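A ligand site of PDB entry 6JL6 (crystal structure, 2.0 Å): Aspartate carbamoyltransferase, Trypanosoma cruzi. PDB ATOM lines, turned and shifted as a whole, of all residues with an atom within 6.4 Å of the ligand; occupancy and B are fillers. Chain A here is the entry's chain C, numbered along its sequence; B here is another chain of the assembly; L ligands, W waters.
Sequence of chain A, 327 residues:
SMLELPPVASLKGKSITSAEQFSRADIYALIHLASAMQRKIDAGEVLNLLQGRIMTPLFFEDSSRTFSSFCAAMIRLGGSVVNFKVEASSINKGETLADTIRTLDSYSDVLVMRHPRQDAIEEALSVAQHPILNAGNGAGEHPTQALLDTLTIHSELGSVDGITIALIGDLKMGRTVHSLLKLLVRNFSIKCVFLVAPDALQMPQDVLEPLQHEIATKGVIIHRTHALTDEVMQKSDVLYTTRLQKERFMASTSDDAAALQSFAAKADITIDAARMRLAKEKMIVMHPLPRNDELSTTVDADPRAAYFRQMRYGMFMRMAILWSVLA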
ATOM      1  N   GLU A  61      19.179   2.222 -19.339  1.00  0.00           N
ATOM      2  CA  GLU A  61      20.068   2.419 -20.472  1.00  0.00           C
ATOM      3  C   GLU A  61      21.251   1.622 -20.005  1.00  0.00           C
ATOM      4  O   GLU A  61      21.545   1.596 -18.801  1.00  0.00           O
ATOM      5  CB  GLU A  61      20.424   3.899 -20.726  1.00  0.00           C
ATOM      6  CG  GLU A  61      21.413   4.531 -19.734  1.00  0.00           C
ATOM      7  CD  GLU A  61      21.507   6.052 -19.814  1.00  0.00           C
ATOM      8  OE1 GLU A  61      22.127   6.660 -18.907  1.00  0.00           O
ATOM      9  OE2 GLU A  61      20.949   6.650 -20.757  1.00  0.00           O
ATOM     10  N   SER A  63      25.295   0.261 -19.834  1.00  0.00           N
ATOM     11  CA  SER A  63      26.685   0.630 -19.854  1.00  0.00           C
ATOM     12  C   SER A  63      27.315  -0.485 -19.021  1.00  0.00           C
ATOM     13  O   SER A  63      27.428  -0.371 -17.797  1.00  0.00           O
ATOM     14  CB  SER A  63      26.898   1.997 -19.206  1.00  0.00           C
ATOM     15  OG  SER A  63      28.267   2.225 -18.875  1.00  0.00           O
ATOM     16  N   ARG A  65      30.229  -1.014 -19.082  1.00  0.00           N
ATOM     17  CA  ARG A  65      31.350  -0.240 -18.569  1.00  0.00           C
ATOM     18  C   ARG A  65      31.199   0.200 -17.093  1.00  0.00           C
ATOM     19  O   ARG A  65      32.085  -0.063 -16.276  1.00  0.00           O
ATOM     20  CB  ARG A  65      31.566   0.999 -19.457  1.00  0.00           C
ATOM     21  CG  ARG A  65      32.784   1.807 -19.101  1.00  0.00           C
ATOM     22  CD  ARG A  65      32.730   3.239 -19.633  1.00  0.00           C
ATOM     23  NE  ARG A  65      33.837   4.012 -19.059  1.00  0.00           N
ATOM     24  CZ  ARG A  65      35.111   3.906 -19.451  1.00  0.00           C
ATOM     25  NH1 ARG A  65      36.046   4.618 -18.846  1.00  0.00           N
ATOM     26  NH2 ARG A  65      35.467   3.084 -20.422  1.00  0.00           N
ATOM     27  N   THR A  66      30.094   0.887 -16.770  1.00  0.00           N
ATOM     28  CA  THR A  66      29.931   1.446 -15.419  1.00  0.00           C
ATOM     29  C   THR A  66      29.569   0.354 -14.411  1.00  0.00           C
ATOM     30  O   THR A  66      30.097   0.353 -13.294  1.00  0.00           O
ATOM     31  CB  THR A  66      28.918   2.610 -15.390  1.00  0.00           C
ATOM     32  OG1 THR A  66      29.380   3.657 -16.249  1.00  0.00           O
ATOM     33  CG2 THR A  66      28.776   3.192 -13.962  1.00  0.00           C
ATOM     34  N   ARG A 114      20.946   2.726 -13.206  1.00  0.00           N
ATOM     35  CA  ARG A 114      21.214   3.708 -14.271  1.00  0.00           C
ATOM     36  C   ARG A 114      19.953   3.743 -15.124  1.00  0.00           C
ATOM     37  O   ARG A 114      19.419   2.668 -15.488  1.00  0.00           O
ATOM     38  CB  ARG A 114      22.458   3.348 -15.107  1.00  0.00           C
ATOM     39  CG  ARG A 114      22.634   4.246 -16.330  1.00  0.00           C
ATOM     40  CD  ARG A 114      23.971   4.115 -17.096  1.00  0.00           C
ATOM     41  NE  ARG A 114      24.997   4.766 -16.321  1.00  0.00           N
ATOM     42  CZ  ARG A 114      26.129   5.278 -16.779  1.00  0.00           C
ATOM     43  NH1 ARG A 114      26.457   5.265 -18.064  1.00  0.00           N
ATOM     44  NH2 ARG A 114      26.939   5.827 -15.892  1.00  0.00           N
ATOM     45  N   ALA A 135      23.708   5.389 -10.337  1.00  0.00           N
ATOM     46  CA  ALA A 135      24.847   5.394 -11.266  1.00  0.00           C
ATOM     47  C   ALA A 135      24.548   6.218 -12.540  1.00  0.00           C
ATOM     48  O   ALA A 135      25.228   6.039 -13.560  1.00  0.00           O
ATOM     49  CB  ALA A 135      25.258   3.970 -11.613  1.00  0.00           C
ATOM     50  N   GLY A 136      23.518   7.074 -12.491  1.00  0.00           N
ATOM     51  CA  GLY A 136      23.215   8.033 -13.545  1.00  0.00           C
ATOM     52  C   GLY A 136      21.737   8.054 -13.870  1.00  0.00           C
ATOM     53  O   GLY A 136      21.175   7.028 -14.287  1.00  0.00           O
ATOM     54  N   GLY A 138      19.479  10.088 -16.334  1.00  0.00           N
ATOM     55  CA  GLY A 138      19.371  11.021 -17.467  1.00  0.00           C
ATOM     56  C   GLY A 138      20.524  12.032 -17.456  1.00  0.00           C
ATOM     57  O   GLY A 138      21.666  11.658 -17.197  1.00  0.00           O
ATOM     58  N   HIS A 142      25.293  12.048 -11.049  1.00  0.00           N
ATOM     59  CA  HIS A 142      26.184  10.914 -11.048  1.00  0.00           C
ATOM     60  C   HIS A 142      27.022  11.088  -9.766  1.00  0.00           C
ATOM     61  O   HIS A 142      28.194  11.447  -9.833  1.00  0.00           O
ATOM     62  CB  HIS A 142      27.033  10.912 -12.328  1.00  0.00           C
ATOM     63  CG  HIS A 142      27.641   9.589 -12.681  1.00  0.00           C
ATOM     64  ND1 HIS A 142      27.797   8.560 -11.773  1.00  0.00           N
ATOM     65  CD2 HIS A 142      28.180   9.148 -13.832  1.00  0.00           C
ATOM     66  CE1 HIS A 142      28.400   7.542 -12.362  1.00  0.00           C
ATOM     67  NE2 HIS A 142      28.646   7.871 -13.622  1.00  0.00           N
ATOM     68  N   GLN A 145      30.484   9.439  -9.077  1.00  0.00           N
ATOM     69  CA  GLN A 145      31.528  10.032  -9.911  1.00  0.00           C
ATOM     70  C   GLN A 145      32.106  11.269  -9.224  1.00  0.00           C
ATOM     71  O   GLN A 145      33.326  11.429  -9.192  1.00  0.00           O
ATOM     72  CB  GLN A 145      31.010  10.379 -11.300  1.00  0.00           C
ATOM     73  CG  GLN A 145      32.113  10.872 -12.241  1.00  0.00           C
ATOM     74  CD  GLN A 145      32.989   9.740 -12.775  1.00  0.00           C
ATOM     75  OE1 GLN A 145      32.471   8.696 -13.135  1.00  0.00           O
ATOM     76  NE2 GLN A 145      34.300   9.955 -12.848  1.00  0.00           N
ATOM     77  N   GLY A 174      25.805  16.957 -19.041  1.00  0.00           N
ATOM     78  CA  GLY A 174      26.811  16.274 -18.253  1.00  0.00           C
ATOM     79  C   GLY A 174      26.457  16.092 -16.787  1.00  0.00           C
ATOM     80  O   GLY A 174      26.820  16.920 -15.929  1.00  0.00           O
ATOM     81  N   ARG A 175      25.787  14.986 -16.481  1.00  0.00           N
ATOM     82  CA  ARG A 175      25.489  14.618 -15.104  1.00  0.00           C
ATOM     83  C   ARG A 175      26.702  14.587 -14.165  1.00  0.00           C
ATOM     84  O   ARG A 175      26.577  14.876 -12.979  1.00  0.00           O
ATOM     85  CB  ARG A 175      24.703  13.314 -15.050  1.00  0.00           C
ATOM     86  CG  ARG A 175      25.341  12.123 -15.728  1.00  0.00           C
ATOM     87  CD  ARG A 175      24.450  10.908 -15.597  1.00  0.00           C
ATOM     88  NE  ARG A 175      24.922   9.811 -16.418  1.00  0.00           N
ATOM     89  CZ  ARG A 175      24.171   8.944 -17.082  1.00  0.00           C
ATOM     90  NH1 ARG A 175      24.767   7.986 -17.772  1.00  0.00           N
ATOM     91  NH2 ARG A 175      22.838   8.989 -17.076  1.00  0.00           N
ATOM     92  N   THR A 176      27.867  14.291 -14.721  1.00  0.00           N
ATOM     93  CA  THR A 176      29.140  14.300 -13.991  1.00  0.00           C
ATOM     94  C   THR A 176      29.489  15.675 -13.434  1.00  0.00           C
ATOM     95  O   THR A 176      29.765  15.823 -12.247  1.00  0.00           O
ATOM     96  CB  THR A 176      30.259  13.865 -14.939  1.00  0.00           C
ATOM     97  OG1 THR A 176      30.190  14.681 -16.144  1.00  0.00           O
ATOM     98  CG2 THR A 176      30.046  12.384 -15.290  1.00  0.00           C
ATOM     99  N   THR A 242      34.746  16.719 -20.814  1.00  0.00           N
ATOM    100  CA  THR A 242      33.637  15.771 -20.976  1.00  0.00           C
ATOM    101  C   THR A 242      33.271  15.509 -22.431  1.00  0.00           C
ATOM    102  O   THR A 242      33.520  16.322 -23.309  1.00  0.00           O
ATOM    103  CB  THR A 242      32.352  16.274 -20.268  1.00  0.00           C
ATOM    104  OG1 THR A 242      31.945  17.519 -20.842  1.00  0.00           O
ATOM    105  CG2 THR A 242      32.537  16.458 -18.760  1.00  0.00           C
ATOM    106  N   ARG A 243      32.610  14.376 -22.624  1.00  0.00           N
ATOM    107  CA  ARG A 243      32.104  13.925 -23.911  1.00  0.00           C
ATOM    108  C   ARG A 243      30.766  14.592 -24.219  1.00  0.00           C
ATOM    109  O   ARG A 243      29.918  14.757 -23.331  1.00  0.00           O
ATOM    110  CB  ARG A 243      31.901  12.423 -23.840  1.00  0.00           C
ATOM    111  CG  ARG A 243      31.368  11.790 -25.119  1.00  0.00           C
ATOM    112  CD  ARG A 243      31.275  10.282 -24.990  1.00  0.00           C
ATOM    113  NE  ARG A 243      30.303   9.889 -23.955  1.00  0.00           N
ATOM    114  CZ  ARG A 243      28.994   9.760 -24.122  1.00  0.00           C
ATOM    115  NH1 ARG A 243      28.390   9.998 -25.292  1.00  0.00           N
ATOM    116  NH2 ARG A 243      28.252   9.404 -23.080  1.00  0.00           N
ATOM    117  N   LEU A 244      30.566  14.942 -25.489  1.00  0.00           N
ATOM    118  CA  LEU A 244      29.253  15.355 -25.984  1.00  0.00           C
ATOM    119  C   LEU A 244      28.235  14.215 -25.818  1.00  0.00           C
ATOM    120  O   LEU A 244      28.415  13.140 -26.361  1.00  0.00           O
ATOM    121  CB  LEU A 244      29.335  15.755 -27.461  1.00  0.00           C
ATOM    122  CG  LEU A 244      28.052  16.258 -28.150  1.00  0.00           C
ATOM    123  CD1 LEU A 244      27.539  17.520 -27.451  1.00  0.00           C
ATOM    124  CD2 LEU A 244      28.322  16.513 -29.630  1.00  0.00           C
ATOM    125  N   GLN A 245      27.159  14.439 -25.073  1.00  0.00           N
ATOM    126  CA  GLN A 245      26.172  13.423 -24.746  1.00  0.00           C
ATOM    127  C   GLN A 245      25.162  13.234 -25.892  1.00  0.00           C
ATOM    128  O   GLN A 245      24.039  13.558 -25.786  1.00  0.00           O
ATOM    129  CB  GLN A 245      25.475  13.774 -23.445  1.00  0.00           C
ATOM    130  CG  GLN A 245      26.391  14.094 -22.291  1.00  0.00           C
ATOM    131  CD  GLN A 245      27.119  12.878 -21.768  1.00  0.00           C
ATOM    132  OE1 GLN A 245      26.517  12.044 -21.158  1.00  0.00           O
ATOM    133  NE2 GLN A 245      28.366  12.786 -22.046  1.00  0.00           N
ATOM    134  N   GLU A 247      23.628  10.756 -27.175  1.00  0.00           N
ATOM    135  CA  GLU A 247      22.468   9.948 -26.732  1.00  0.00           C
ATOM    136  C   GLU A 247      21.314  10.789 -26.177  1.00  0.00           C
ATOM    137  O   GLU A 247      20.163  10.378 -26.257  1.00  0.00           O
ATOM    138  CB  GLU A 247      22.841   8.886 -25.647  1.00  0.00           C
ATOM    139  CG  GLU A 247      24.311   8.497 -25.421  1.00  0.00           C
ATOM    140  CD  GLU A 247      24.978   9.289 -24.308  1.00  0.00           C
ATOM    141  OE1 GLU A 247      25.001  10.525 -24.396  1.00  0.00           O
ATOM    142  OE2 GLU A 247      25.479   8.694 -23.333  1.00  0.00           O
ATOM    143  N   ARG A 248      21.620  11.942 -25.574  1.00  0.00           N
ATOM    144  CA  ARG A 248      20.609  12.899 -25.090  1.00  0.00           C
ATOM    145  C   ARG A 248      19.959  13.777 -26.166  1.00  0.00           C
ATOM    146  O   ARG A 248      19.013  14.528 -25.869  1.00  0.00           O
ATOM    147  CB  ARG A 248      21.216  13.831 -24.022  1.00  0.00           C
ATOM    148  CG  ARG A 248      20.881  13.478 -22.593  1.00  0.00           C
ATOM    149  CD  ARG A 248      21.700  12.334 -22.037  1.00  0.00           C
ATOM    150  NE  ARG A 248      20.869  11.163 -21.804  1.00  0.00           N
ATOM    151  CZ  ARG A 248      21.208  10.107 -21.059  1.00  0.00           C
ATOM    152  NH1 ARG A 248      22.404   9.995 -20.471  1.00  0.00           N
ATOM    153  NH2 ARG A 248      20.331   9.130 -20.936  1.00  0.00           N
ATOM    154  N   HIS A 287      38.810  13.508 -16.929  1.00  0.00           N
ATOM    155  CA  HIS A 287      37.699  13.180 -17.839  1.00  0.00           C
ATOM    156  C   HIS A 287      36.998  11.964 -17.201  1.00  0.00           C
ATOM    157  O   HIS A 287      37.657  10.963 -16.930  1.00  0.00           O
ATOM    158  CB  HIS A 287      38.234  12.832 -19.247  1.00  0.00           C
ATOM    159  CG  HIS A 287      37.177  12.829 -20.318  1.00  0.00           C
ATOM    160  ND1 HIS A 287      35.967  12.193 -20.170  1.00  0.00           N
ATOM    161  CD2 HIS A 287      37.147  13.392 -21.550  1.00  0.00           C
ATOM    162  CE1 HIS A 287      35.236  12.353 -21.252  1.00  0.00           C
ATOM    163  NE2 HIS A 287      35.925  13.083 -22.103  1.00  0.00           N
ATOM    164  N   PRO A 288      35.666  12.046 -16.973  1.00  0.00           N
ATOM    165  CA  PRO A 288      34.963  10.873 -16.399  1.00  0.00           C
ATOM    166  C   PRO A 288      34.997   9.614 -17.235  1.00  0.00           C
ATOM    167  O   PRO A 288      34.897   8.536 -16.704  1.00  0.00           O
ATOM    168  CB  PRO A 288      33.507  11.345 -16.282  1.00  0.00           C
ATOM    169  CG  PRO A 288      33.387  12.513 -17.227  1.00  0.00           C
ATOM    170  CD  PRO A 288      34.751  13.163 -17.260  1.00  0.00           C
ATOM    171  N   LEU A 289      35.017   9.812 -18.554  1.00  0.00           N
ATOM    172  CA  LEU A 289      35.187   8.812 -19.601  1.00  0.00           C
ATOM    173  C   LEU A 289      33.817   8.156 -19.856  1.00  0.00           C
ATOM    174  O   LEU A 289      32.953   8.214 -18.973  1.00  0.00           O
ATOM    175  CB  LEU A 289      36.318   7.781 -19.344  1.00  0.00           C
ATOM    176  CG  LEU A 289      37.750   8.326 -19.368  1.00  0.00           C
ATOM    177  CD1 LEU A 289      38.718   7.214 -19.032  1.00  0.00           C
ATOM    178  CD2 LEU A 289      38.135   8.982 -20.698  1.00  0.00           C
ATOM    179  N   PRO A 290      33.576   7.615 -21.045  1.00  0.00           N
ATOM    180  CA  PRO A 290      34.504   7.586 -22.162  1.00  0.00           C
ATOM    181  C   PRO A 290      34.602   8.921 -22.878  1.00  0.00           C
ATOM    182  O   PRO A 290      33.732   9.778 -22.731  1.00  0.00           O
ATOM    183  CB  PRO A 290      33.861   6.573 -23.110  1.00  0.00           C
ATOM    184  CG  PRO A 290      32.405   6.757 -22.872  1.00  0.00           C
ATOM    185  CD  PRO A 290      32.290   6.991 -21.396  1.00  0.00           C
ATOM    186  N   ARG A 291      35.663   9.048 -23.664  1.00  0.00           N
ATOM    187  CA  ARG A 291      35.966  10.258 -24.426  1.00  0.00           C
ATOM    188  C   ARG A 291      35.841  10.001 -25.923  1.00  0.00           C
ATOM    189  O   ARG A 291      35.917   8.852 -26.363  1.00  0.00           O
ATOM    190  CB  ARG A 291      37.397  10.732 -24.140  1.00  0.00           C
ATOM    191  CG  ARG A 291      38.468   9.721 -24.552  1.00  0.00           C
ATOM    192  CD  ARG A 291      39.875  10.266 -24.578  1.00  0.00           C
ATOM    193  NE  ARG A 291      40.807   9.156 -24.605  1.00  0.00           N
ATOM    194  CZ  ARG A 291      42.124   9.274 -24.655  1.00  0.00           C
ATOM    195  NH1 ARG A 291      42.718  10.474 -24.761  1.00  0.00           N
ATOM    196  NH2 ARG A 291      42.863   8.175 -24.642  1.00  0.00           N
ATOM    197  N   LYS B  93      28.981   4.839 -27.797  1.00  0.00           N
ATOM    198  CA  LYS B  93      29.454   6.179 -27.428  1.00  0.00           C
ATOM    199  C   LYS B  93      30.853   6.508 -27.995  1.00  0.00           C
ATOM    200  O   LYS B  93      31.450   7.524 -27.617  1.00  0.00           O
ATOM    201  CB  LYS B  93      29.485   6.329 -25.898  1.00  0.00           C
ATOM    202  CG  LYS B  93      28.209   5.945 -25.160  1.00  0.00           C
ATOM    203  CD  LYS B  93      28.496   5.837 -23.657  1.00  0.00           C
ATOM    204  CE  LYS B  93      27.385   5.152 -22.862  1.00  0.00           C
ATOM    205  NZ  LYS B  93      26.533   6.112 -22.113  1.00  0.00           N
HETATM  206  N1  LIG L   1      30.430   7.771 -18.104  1.00  0.00           N
HETATM  207  C1  LIG L   1      29.922   9.087 -17.678  1.00  0.00           C
HETATM  208  C2  LIG L   1      28.412   8.997 -17.451  1.00  0.00           C
HETATM  209  O1  LIG L   1      27.865   7.887 -17.444  1.00  0.00           O
HETATM  210  C3  LIG L   1      30.311  10.214 -18.674  1.00  0.00           C
HETATM  211  C4  LIG L   1      29.928   9.904 -20.127  1.00  0.00           C
HETATM  212  O2  LIG L   1      29.189   8.930 -20.398  1.00  0.00           O
HETATM  213  O3  LIG L   1      30.385  10.669 -21.028  1.00  0.00           O
HETATM  214  O4  LIG L   1      27.718   9.986 -17.248  1.00  0.00           O
HETATM  215  O   HOH W   1      31.904  12.760 -20.403  1.00  0.00           O
HETATM  216  O   HOH W   2      32.151   7.826 -15.826  1.00  0.00           O
HETATM  217  O   HOH W   3      27.539  12.498 -18.361  1.00  0.00           O
HETATM  218  O   HOH W   4      29.738   6.197 -15.632  1.00  0.00           O
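Water W1 lies within hydrogen-bond range of an oxygen (O3) of the ligand (2.7 Å) and the backbone NH (N) of Arg 243 (2.8 Å).
Water W3 lies within hydrogen-bond range of O4 of the ligand and OE1 of Gln 245.
Water W4 lies within hydrogen-bond range of OG1 of Thr 66 (2.6 Å), NE2 of His 142 (2.8 Å), NH2 of Arg 114 (2.8 Å) and N1 of the ligand (3.0 Å).
His 142 touches the ligand (CD2 to O4, 3.5 Å).
CG2 of Thr 176 touches O4 of the ligand, 3.9 Å away.
CD of Pro 290 touches O2 of the ligand, at 3.8 Å.
Hydrophobic or aromatic side chains within 4 Å of the ligand: His 142 and Pro 290.
Of the 25 residues printed, 8 come within 4 Å of the ligand.
The nearest printed residue that does not touch the ligand is Pro 288 (4.1 Å).
The backbone carbonyl oxygen of Arg 243 lies within hydrogen-bond range of the side-chain amide nitrogen of Gln 245.
OE1 of Glu 61 lies within salt-bridge range of NH2 of Arg 175 (3.0 Å).
The guanidinium group of Arg 114 sits at hydrogen-bond distance from the backbone carbonyl oxygen of Ala 135, 2.9 Å away.
The backbone carbonyl oxygen of Gly 138 sits at hydrogen-bond distance from the guanidinium group of Arg 175 (2.9 Å).
The backbone NH of Leu 289 lies within hydrogen-bond range of a ring nitrogen (ND1) of His 287 (3.0 Å).
The side-chain hydroxyl of Thr 66 is in hydrogen-bond range of the guanidinium group of Arg 114, 3.3 Å away.
The side-chain carboxylate of Glu 247 is in salt-bridge range of the guanidinium group of Arg 243, 2.9 Å away.
NH2 of Arg 114 lies within hydrogen-bond range of NE2 of His 142.
An oxygen (O4) of the ligand is in salt-bridge range of the guanidinium group (NE) of Arg 175.
NH2 of Arg 114 lies within salt-bridge range of O1 of the ligand, at 2.7 Å.
The guanidinium group of Arg 243 lies within salt-bridge range of an oxygen (O2) of the ligand (2.9 Å).
A nitrogen (N1) of the ligand lies within hydrogen-bond range of the backbone carbonyl oxygen of Leu 289, 2.7 Å away.
The side-chain amide nitrogen of Gln 245 is in hydrogen-bond range of an oxygen (O3) of the ligand, at 3.1 Å.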
